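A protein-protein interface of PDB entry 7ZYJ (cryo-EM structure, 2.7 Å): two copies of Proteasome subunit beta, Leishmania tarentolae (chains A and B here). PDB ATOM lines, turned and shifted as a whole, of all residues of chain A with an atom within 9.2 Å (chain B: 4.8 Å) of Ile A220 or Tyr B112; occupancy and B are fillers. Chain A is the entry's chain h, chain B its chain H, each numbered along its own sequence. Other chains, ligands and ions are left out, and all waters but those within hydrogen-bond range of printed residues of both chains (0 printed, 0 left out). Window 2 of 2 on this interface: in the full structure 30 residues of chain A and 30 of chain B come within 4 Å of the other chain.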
ATOM      1  N   GLN A 207      -1.384  -1.009   7.974  1.00  0.00           N
ATOM      2  CA  GLN A 207      -0.327  -1.144   8.962  1.00  0.00           C
ATOM      3  C   GLN A 207      -0.862  -1.753  10.252  1.00  0.00           C
ATOM      4  O   GLN A 207      -2.027  -1.572  10.614  1.00  0.00           O
ATOM      5  CB  GLN A 207       0.313   0.213   9.255  1.00  0.00           C
ATOM      6  CG  GLN A 207       1.463   0.564   8.333  1.00  0.00           C
ATOM      7  CD  GLN A 207       2.140   1.861   8.715  1.00  0.00           C
ATOM      8  OE1 GLN A 207       1.496   2.792   9.195  1.00  0.00           O
ATOM      9  NE2 GLN A 207       3.450   1.924   8.517  1.00  0.00           N
ATOM     10  N   ALA A 208       0.007  -2.490  10.941  1.00  0.00           N
ATOM     11  CA  ALA A 208      -0.351  -3.044  12.238  1.00  0.00           C
ATOM     12  C   ALA A 208      -0.630  -1.922  13.230  1.00  0.00           C
ATOM     13  O   ALA A 208       0.032  -0.882  13.221  1.00  0.00           O
ATOM     14  CB  ALA A 208       0.770  -3.942  12.759  1.00  0.00           C
ATOM     15  N   THR A 209      -1.625  -2.133  14.086  1.00  0.00           N
ATOM     16  CA  THR A 209      -2.053  -1.109  15.037  1.00  0.00           C
ATOM     17  C   THR A 209      -1.182  -1.210  16.283  1.00  0.00           C
ATOM     18  O   THR A 209      -1.480  -1.952  17.221  1.00  0.00           O
ATOM     19  CB  THR A 209      -3.527  -1.271  15.375  1.00  0.00           C
ATOM     20  OG1 THR A 209      -4.272  -1.471  14.168  1.00  0.00           O
ATOM     21  CG2 THR A 209      -4.034  -0.021  16.041  1.00  0.00           C
ATOM     22  N   GLN A 210      -0.094  -0.447  16.295  1.00  0.00           N
ATOM     23  CA  GLN A 210       0.881  -0.483  17.378  1.00  0.00           C
ATOM     24  C   GLN A 210       0.934   0.799  18.192  1.00  0.00           C
ATOM     25  O   GLN A 210       1.143   0.744  19.405  1.00  0.00           O
ATOM     26  CB  GLN A 210       2.276  -0.771  16.815  1.00  0.00           C
ATOM     27  CG  GLN A 210       2.406  -2.116  16.124  1.00  0.00           C
ATOM     28  CD  GLN A 210       2.271  -3.281  17.079  1.00  0.00           C
ATOM     29  OE1 GLN A 210       1.288  -4.018  17.042  1.00  0.00           O
ATOM     30  NE2 GLN A 210       3.264  -3.456  17.941  1.00  0.00           N
ATOM     31  N   ASN A 211       0.764   1.957  17.554  1.00  0.00           N
ATOM     32  CA  ASN A 211       0.897   3.250  18.224  1.00  0.00           C
ATOM     33  C   ASN A 211      -0.489   3.762  18.603  1.00  0.00           C
ATOM     34  O   ASN A 211      -1.064   4.634  17.953  1.00  0.00           O
ATOM     35  CB  ASN A 211       1.641   4.238  17.332  1.00  0.00           C
ATOM     36  CG  ASN A 211       2.904   3.650  16.745  1.00  0.00           C
ATOM     37  OD1 ASN A 211       3.541   2.788  17.347  1.00  0.00           O
ATOM     38  ND2 ASN A 211       3.276   4.118  15.561  1.00  0.00           N
ATOM     39  N   GLN A 212      -1.021   3.207  19.688  1.00  0.00           N
ATOM     40  CA  GLN A 212      -2.339   3.604  20.158  1.00  0.00           C
ATOM     41  C   GLN A 212      -2.329   5.068  20.595  1.00  0.00           C
ATOM     42  O   GLN A 212      -1.417   5.498  21.307  1.00  0.00           O
ATOM     43  CB  GLN A 212      -2.771   2.732  21.335  1.00  0.00           C
ATOM     44  CG  GLN A 212      -2.952   1.259  21.027  1.00  0.00           C
ATOM     45  CD  GLN A 212      -4.097   0.996  20.080  1.00  0.00           C
ATOM     46  OE1 GLN A 212      -4.011   0.134  19.207  1.00  0.00           O
ATOM     47  NE2 GLN A 212      -5.164   1.765  20.222  1.00  0.00           N
ATOM     48  N   PRO A 213      -3.314   5.856  20.176  1.00  0.00           N
ATOM     49  CA  PRO A 213      -3.512   7.166  20.800  1.00  0.00           C
ATOM     50  C   PRO A 213      -3.980   6.998  22.235  1.00  0.00           C
ATOM     51  O   PRO A 213      -4.632   6.012  22.587  1.00  0.00           O
ATOM     52  CB  PRO A 213      -4.595   7.820  19.933  1.00  0.00           C
ATOM     53  CG  PRO A 213      -4.620   7.030  18.664  1.00  0.00           C
ATOM     54  CD  PRO A 213      -4.228   5.638  19.044  1.00  0.00           C
ATOM     55  N   SER A 215      -6.323   7.148  24.981  1.00  0.00           N
ATOM     56  CA  SER A 215      -7.774   7.133  24.898  1.00  0.00           C
ATOM     57  C   SER A 215      -8.377   6.729  26.236  1.00  0.00           C
ATOM     58  O   SER A 215      -7.724   6.111  27.080  1.00  0.00           O
ATOM     59  CB  SER A 215      -8.263   6.178  23.800  1.00  0.00           C
ATOM     60  OG  SER A 215      -8.223   4.834  24.243  1.00  0.00           O
ATOM     61  N   SER A 217     -10.920   4.689  26.392  1.00  0.00           N
ATOM     62  CA  SER A 217     -11.579   3.416  26.155  1.00  0.00           C
ATOM     63  C   SER A 217     -10.563   2.367  25.728  1.00  0.00           C
ATOM     64  O   SER A 217      -9.463   2.684  25.268  1.00  0.00           O
ATOM     65  CB  SER A 217     -12.670   3.547  25.085  1.00  0.00           C
ATOM     66  OG  SER A 217     -13.454   2.371  25.010  1.00  0.00           O
ATOM     67  N   ALA A 218     -10.950   1.104  25.887  1.00  0.00           N
ATOM     68  CA  ALA A 218     -10.146  -0.024  25.442  1.00  0.00           C
ATOM     69  C   ALA A 218     -10.355  -0.351  23.970  1.00  0.00           C
ATOM     70  O   ALA A 218      -9.716  -1.274  23.456  1.00  0.00           O
ATOM     71  CB  ALA A 218     -10.453  -1.260  26.293  1.00  0.00           C
ATOM     72  N   LYS A 219     -11.234   0.378  23.287  1.00  0.00           N
ATOM     73  CA  LYS A 219     -11.472   0.148  21.868  1.00  0.00           C
ATOM     74  C   LYS A 219     -10.247   0.542  21.052  1.00  0.00           C
ATOM     75  O   LYS A 219      -9.712   1.643  21.207  1.00  0.00           O
ATOM     76  CB  LYS A 219     -12.694   0.942  21.406  1.00  0.00           C
ATOM     77  CG  LYS A 219     -13.037   0.777  19.935  1.00  0.00           C
ATOM     78  CD  LYS A 219     -13.512  -0.629  19.622  1.00  0.00           C
ATOM     79  CE  LYS A 219     -14.000  -0.736  18.187  1.00  0.00           C
ATOM     80  NZ  LYS A 219     -12.897  -0.546  17.205  1.00  0.00           N
ATOM     81  N   ILE A 220      -9.811  -0.358  20.178  1.00  0.00           N
ATOM     82  CA  ILE A 220      -8.672  -0.091  19.308  1.00  0.00           C
ATOM     83  C   ILE A 220      -9.166   0.632  18.063  1.00  0.00           C
ATOM     84  O   ILE A 220     -10.054   0.140  17.356  1.00  0.00           O
ATOM     85  CB  ILE A 220      -7.947  -1.397  18.948  1.00  0.00           C
ATOM     86  CG1 ILE A 220      -7.290  -1.996  20.192  1.00  0.00           C
ATOM     87  CG2 ILE A 220      -6.913  -1.150  17.871  1.00  0.00           C
ATOM     88  CD1 ILE A 220      -6.925  -3.453  20.047  1.00  0.00           C
ATOM     89  N   THR A 221      -8.591   1.807  17.789  1.00  0.00           N
ATOM     90  CA  THR A 221      -9.097   2.687  16.740  1.00  0.00           C
ATOM     91  C   THR A 221      -8.006   3.142  15.776  1.00  0.00           C
ATOM     92  O   THR A 221      -8.123   4.220  15.186  1.00  0.00           O
ATOM     93  CB  THR A 221      -9.787   3.913  17.346  1.00  0.00           C
ATOM     94  OG1 THR A 221      -8.878   4.588  18.224  1.00  0.00           O
ATOM     95  CG2 THR A 221     -11.030   3.504  18.122  1.00  0.00           C
ATOM     96  N   GLY A 222      -6.950   2.354  15.602  1.00  0.00           N
ATOM     97  CA  GLY A 222      -5.908   2.698  14.656  1.00  0.00           C
ATOM     98  C   GLY A 222      -4.713   3.374  15.298  1.00  0.00           C
ATOM     99  O   GLY A 222      -4.677   3.673  16.494  1.00  0.00           O
ATOM    100  N   ASN A 223      -3.707   3.615  14.464  1.00  0.00           N
ATOM    101  CA  ASN A 223      -2.471   4.236  14.915  1.00  0.00           C
ATOM    102  C   ASN A 223      -2.615   5.750  14.994  1.00  0.00           C
ATOM    103  O   ASN A 223      -3.433   6.358  14.298  1.00  0.00           O
ATOM    104  CB  ASN A 223      -1.314   3.877  13.982  1.00  0.00           C
ATOM    105  CG  ASN A 223      -0.878   2.438  14.126  1.00  0.00           C
ATOM    106  OD1 ASN A 223      -0.616   1.966  15.230  1.00  0.00           O
ATOM    107  ND2 ASN A 223      -0.798   1.729  13.007  1.00  0.00           N
ATOM    108  N   VAL B  76      -8.517  -9.238  24.636  1.00  0.00           N
ATOM    109  CA  VAL B  76      -7.336  -9.971  24.192  1.00  0.00           C
ATOM    110  C   VAL B  76      -6.078  -9.143  24.421  1.00  0.00           C
ATOM    111  O   VAL B  76      -4.995  -9.695  24.663  1.00  0.00           O
ATOM    112  CB  VAL B  76      -7.486 -10.382  22.716  1.00  0.00           C
ATOM    113  CG1 VAL B  76      -6.389 -11.357  22.316  1.00  0.00           C
ATOM    114  CG2 VAL B  76      -8.854 -10.990  22.476  1.00  0.00           C
ATOM    115  N   ALA B  77      -6.196  -7.814  24.359  1.00  0.00           N
ATOM    116  CA  ALA B  77      -5.042  -6.951  24.575  1.00  0.00           C
ATOM    117  C   ALA B  77      -4.477  -7.103  25.981  1.00  0.00           C
ATOM    118  O   ALA B  77      -3.262  -7.000  26.171  1.00  0.00           O
ATOM    119  CB  ALA B  77      -5.417  -5.495  24.309  1.00  0.00           C
ATOM    120  N   ALA B  80      -2.431 -10.259  25.970  1.00  0.00           N
ATOM    121  CA  ALA B  80      -1.228  -9.993  25.192  1.00  0.00           C
ATOM    122  C   ALA B  80      -0.226  -9.174  25.995  1.00  0.00           C
ATOM    123  O   ALA B  80       0.975  -9.453  25.967  1.00  0.00           O
ATOM    124  CB  ALA B  80      -1.591  -9.274  23.894  1.00  0.00           C
ATOM    125  N   ILE B  98       5.146 -16.983  21.639  1.00  0.00           N
ATOM    126  CA  ILE B  98       3.751 -17.047  22.047  1.00  0.00           C
ATOM    127  C   ILE B  98       2.892 -16.364  20.994  1.00  0.00           C
ATOM    128  O   ILE B  98       3.280 -15.338  20.426  1.00  0.00           O
ATOM    129  CB  ILE B  98       3.542 -16.400  23.433  1.00  0.00           C
ATOM    130  CG1 ILE B  98       4.466 -17.049  24.465  1.00  0.00           C
ATOM    131  CG2 ILE B  98       2.093 -16.521  23.877  1.00  0.00           C
ATOM    132  CD1 ILE B  98       4.255 -18.538  24.621  1.00  0.00           C
ATOM    133  N   ILE B  99       1.739 -16.955  20.711  1.00  0.00           N
ATOM    134  CA  ILE B  99       0.694 -16.306  19.932  1.00  0.00           C
ATOM    135  C   ILE B  99      -0.532 -16.216  20.824  1.00  0.00           C
ATOM    136  O   ILE B  99      -1.009 -17.236  21.326  1.00  0.00           O
ATOM    137  CB  ILE B  99       0.382 -17.069  18.636  1.00  0.00           C
ATOM    138  CG1 ILE B  99       1.544 -16.944  17.649  1.00  0.00           C
ATOM    139  CG2 ILE B  99      -0.900 -16.549  18.015  1.00  0.00           C
ATOM    140  CD1 ILE B  99       1.403 -17.824  16.428  1.00  0.00           C
ATOM    141  N   VAL B 100      -1.040 -15.008  21.027  1.00  0.00           N
ATOM    142  CA  VAL B 100      -2.214 -14.789  21.863  1.00  0.00           C
ATOM    143  C   VAL B 100      -3.365 -14.413  20.948  1.00  0.00           C
ATOM    144  O   VAL B 100      -3.346 -13.345  20.326  1.00  0.00           O
ATOM    145  CB  VAL B 100      -1.967 -13.701  22.919  1.00  0.00           C
ATOM    146  CG1 VAL B 100      -3.279 -13.269  23.555  1.00  0.00           C
ATOM    147  CG2 VAL B 100      -0.996 -14.199  23.966  1.00  0.00           C
ATOM    148  N   ASN B 107     -13.323  -5.476  20.810  1.00  0.00           N
ATOM    149  CA  ASN B 107     -12.446  -5.409  19.646  1.00  0.00           C
ATOM    150  C   ASN B 107     -12.621  -6.588  18.697  1.00  0.00           C
ATOM    151  O   ASN B 107     -11.837  -6.727  17.752  1.00  0.00           O
ATOM    152  CB  ASN B 107     -10.985  -5.313  20.093  1.00  0.00           C
ATOM    153  CG  ASN B 107     -10.663  -3.985  20.745  1.00  0.00           C
ATOM    154  OD1 ASN B 107     -10.801  -2.930  20.129  1.00  0.00           O
ATOM    155  ND2 ASN B 107     -10.227  -4.032  21.996  1.00  0.00           N
ATOM    156  N   SER B 110      -8.887 -10.898  17.849  1.00  0.00           N
ATOM    157  CA  SER B 110      -7.561 -10.303  17.874  1.00  0.00           C
ATOM    158  C   SER B 110      -6.498 -11.391  17.893  1.00  0.00           C
ATOM    159  O   SER B 110      -6.677 -12.453  18.499  1.00  0.00           O
ATOM    160  CB  SER B 110      -7.383  -9.380  19.087  1.00  0.00           C
ATOM    161  OG  SER B 110      -8.245  -8.259  19.007  1.00  0.00           O
ATOM    162  N   VAL B 111      -5.387 -11.103  17.214  1.00  0.00           N
ATOM    163  CA  VAL B 111      -4.215 -11.970  17.158  1.00  0.00           C
ATOM    164  C   VAL B 111      -2.980 -11.132  17.463  1.00  0.00           C
ATOM    165  O   VAL B 111      -2.764 -10.084  16.842  1.00  0.00           O
ATOM    166  CB  VAL B 111      -4.073 -12.661  15.788  1.00  0.00           C
ATOM    167  CG1 VAL B 111      -2.719 -13.338  15.670  1.00  0.00           C
ATOM    168  CG2 VAL B 111      -5.179 -13.675  15.587  1.00  0.00           C
ATOM    169  N   TYR B 112      -2.167 -11.600  18.408  1.00  0.00           N
ATOM    170  CA  TYR B 112      -0.943 -10.935  18.826  1.00  0.00           C
ATOM    171  C   TYR B 112       0.205 -11.928  18.763  1.00  0.00           C
ATOM    172  O   TYR B 112       0.055 -13.086  19.160  1.00  0.00           O
ATOM    173  CB  TYR B 112      -1.058 -10.387  20.256  1.00  0.00           C
ATOM    174  CG  TYR B 112      -1.992  -9.213  20.411  1.00  0.00           C
ATOM    175  CD1 TYR B 112      -3.352  -9.407  20.607  1.00  0.00           C
ATOM    176  CD2 TYR B 112      -1.514  -7.912  20.381  1.00  0.00           C
ATOM    177  CE1 TYR B 112      -4.211  -8.338  20.757  1.00  0.00           C
ATOM    178  CE2 TYR B 112      -2.365  -6.837  20.532  1.00  0.00           C
ATOM    179  CZ  TYR B 112      -3.712  -7.056  20.720  1.00  0.00           C
ATOM    180  OH  TYR B 112      -4.563  -5.988  20.869  1.00  0.00           O
ATOM    181  N   SER B 113       1.348 -11.469  18.271  1.00  0.00           N
ATOM    182  CA  SER B 113       2.567 -12.261  18.224  1.00  0.00           C
ATOM    183  C   SER B 113       3.556 -11.712  19.240  1.00  0.00           C
ATOM    184  O   SER B 113       3.806 -10.501  19.278  1.00  0.00           O
ATOM    185  CB  SER B 113       3.178 -12.247  16.822  1.00  0.00           C
ATOM    186  OG  SER B 113       4.346 -13.047  16.767  1.00  0.00           O
ATOM    187  N   ILE B 114       4.096 -12.599  20.071  1.00  0.00           N
ATOM    188  CA  ILE B 114       5.134 -12.274  21.042  1.00  0.00           C
ATOM    189  C   ILE B 114       6.317 -13.194  20.769  1.00  0.00           C
ATOM    190  O   ILE B 114       6.337 -14.341  21.242  1.00  0.00           O
ATOM    191  CB  ILE B 114       4.612 -12.411  22.480  1.00  0.00           C
ATOM    192  CG1 ILE B 114       3.390 -11.514  22.678  1.00  0.00           C
ATOM    193  CG2 ILE B 114       5.698 -12.066  23.484  1.00  0.00           C
ATOM    194  CD1 ILE B 114       2.320 -12.118  23.542  1.00  0.00           C
ATOM    195  N   CYS B 120       5.530  -7.325  21.151  1.00  0.00           N
ATOM    196  CA  CYS B 120       4.128  -7.687  20.971  1.00  0.00           C
ATOM    197  C   CYS B 120       3.600  -6.941  19.759  1.00  0.00           C
ATOM    198  O   CYS B 120       3.604  -5.707  19.744  1.00  0.00           O
ATOM    199  CB  CYS B 120       3.304  -7.348  22.216  1.00  0.00           C
ATOM    200  SG  CYS B 120       1.610  -7.972  22.186  1.00  0.00           S
ATOM    201  N   VAL B 121       3.157  -7.680  18.746  1.00  0.00           N
ATOM    202  CA  VAL B 121       2.665  -7.094  17.504  1.00  0.00           C
ATOM    203  C   VAL B 121       1.256  -7.605  17.246  1.00  0.00           C
ATOM    204  O   VAL B 121       1.021  -8.816  17.254  1.00  0.00           O
ATOM    205  CB  VAL B 121       3.587  -7.420  16.316  1.00  0.00           C
ATOM    206  CG1 VAL B 121       3.130  -6.675  15.081  1.00  0.00           C
ATOM    207  CG2 VAL B 121       5.027  -7.068  16.647  1.00  0.00           C
ATOM    208  N   LYS B 122       0.328  -6.685  17.003  1.00  0.00           N
ATOM    209  CA  LYS B 122      -1.044  -7.043  16.666  1.00  0.00           C
ATOM    210  C   LYS B 122      -1.137  -7.251  15.160  1.00  0.00           C
ATOM    211  O   LYS B 122      -0.828  -6.340  14.384  1.00  0.00           O
ATOM    212  CB  LYS B 122      -2.014  -5.957  17.127  1.00  0.00           C
ATOM    213  CG  LYS B 122      -3.475  -6.360  17.057  1.00  0.00           C
ATOM    214  CD  LYS B 122      -4.374  -5.253  17.581  1.00  0.00           C
ATOM    215  CE  LYS B 122      -5.760  -5.333  16.968  1.00  0.00           C
ATOM    216  NZ  LYS B 122      -6.289  -6.724  16.971  1.00  0.00           N
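The backbone NH (N) of Lys B122 lies within hydrogen-bond range of the side-chain amide oxygen (OE1) of Gln A210 (2.8 Å). ND2 of Asn B107 sits at hydrogen-bond distance from O of Ala A218, at 3.2 Å. The side-chain amide nitrogen (NE2) of Gln A210 is in hydrogen-bond range of the backbone carbonyl oxygen (O) of Cys B120. The backbone NH (N) of Ile A220 sits at hydrogen-bond distance from the side-chain amide oxygen (OD1) of Asn B107 (2.8 Å).
O of Val B100 sits at hydrogen-bond distance from N of Tyr B112. The side-chain hydroxyl of Ser B110 sits at hydrogen-bond distance from the side-chain amino group of Lys B122 (3.2 Å). N of Gln A210 is in hydrogen-bond range of OD1 of Asn A223, at 2.7 Å. The backbone NH of Lys A219 lies close to the side-chain hydroxyl of Ser A217, at 3.4 Å. The backbone carbonyl oxygen (O) of Ala A208 sits at hydrogen-bond distance from the side-chain amide nitrogen (ND2) of Asn A223 (2.7 Å). The backbone NH of Ser B113 lies within hydrogen-bond range of the backbone carbonyl oxygen of Val B121, at 2.9 Å.
Among the printed residues, merely in contact across the chains: Ala A208 with Lys B122, Gln A210 with Val B121, Lys A219 with Asn B107, Ile A220 with Tyr B112 and Ile A220 with Lys B122.
Of chain B, only Asn B107 (2.8 Å), Tyr B112 (3.6 Å) and Lys B122 (3.8 Å) come within 4 Å of Ile A220. Of chain A, only Ile A220 (3.6 Å) comes within 4 Å of Tyr B112. No residue of chain A comes within 4 Å of Val B100. No residue of chain A comes within 4 Å of Val B111. No residue of chain A comes within 4 Å of Ser B113. Of the printed residues of chain A, Cys B120 touches Gln A210. Of the printed residues of chain B, Lys A219 touches Asn B107. Of the printed residues of chain B, Ala A218 touches Asn B107. Of the printed residues of chain B, Gln A210 touches Cys B120, Val B121 and Lys B122. Pro A213 touches none of the printed residues of chain B. Ser B110 touches none of the printed residues of chain A. The nearest residue of chain A that does not touch Tyr B112 is Gln A210 (5.8 Å).
Hydrophobic or aromatic side chains of chain A within 4 Å of the printed part of chain B: Ala A208 and Ile A220. Of the 15 printed residues of chain B, 5 touch a printed residue of chain A. Hydrophobic or aromatic side chains of chain B within 4 Å of the printed part of chain A: Tyr B112 and Val B121. Among the printed residues, no Asp or Glu carboxylate lies within 4 Å of a Lys or Arg side-chain nitrogen of the other chain.
No position is printed for both chains. Of the 9 pairs that touch across the chains among the printed residues, none has its exchanged pair printed and touching as well.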
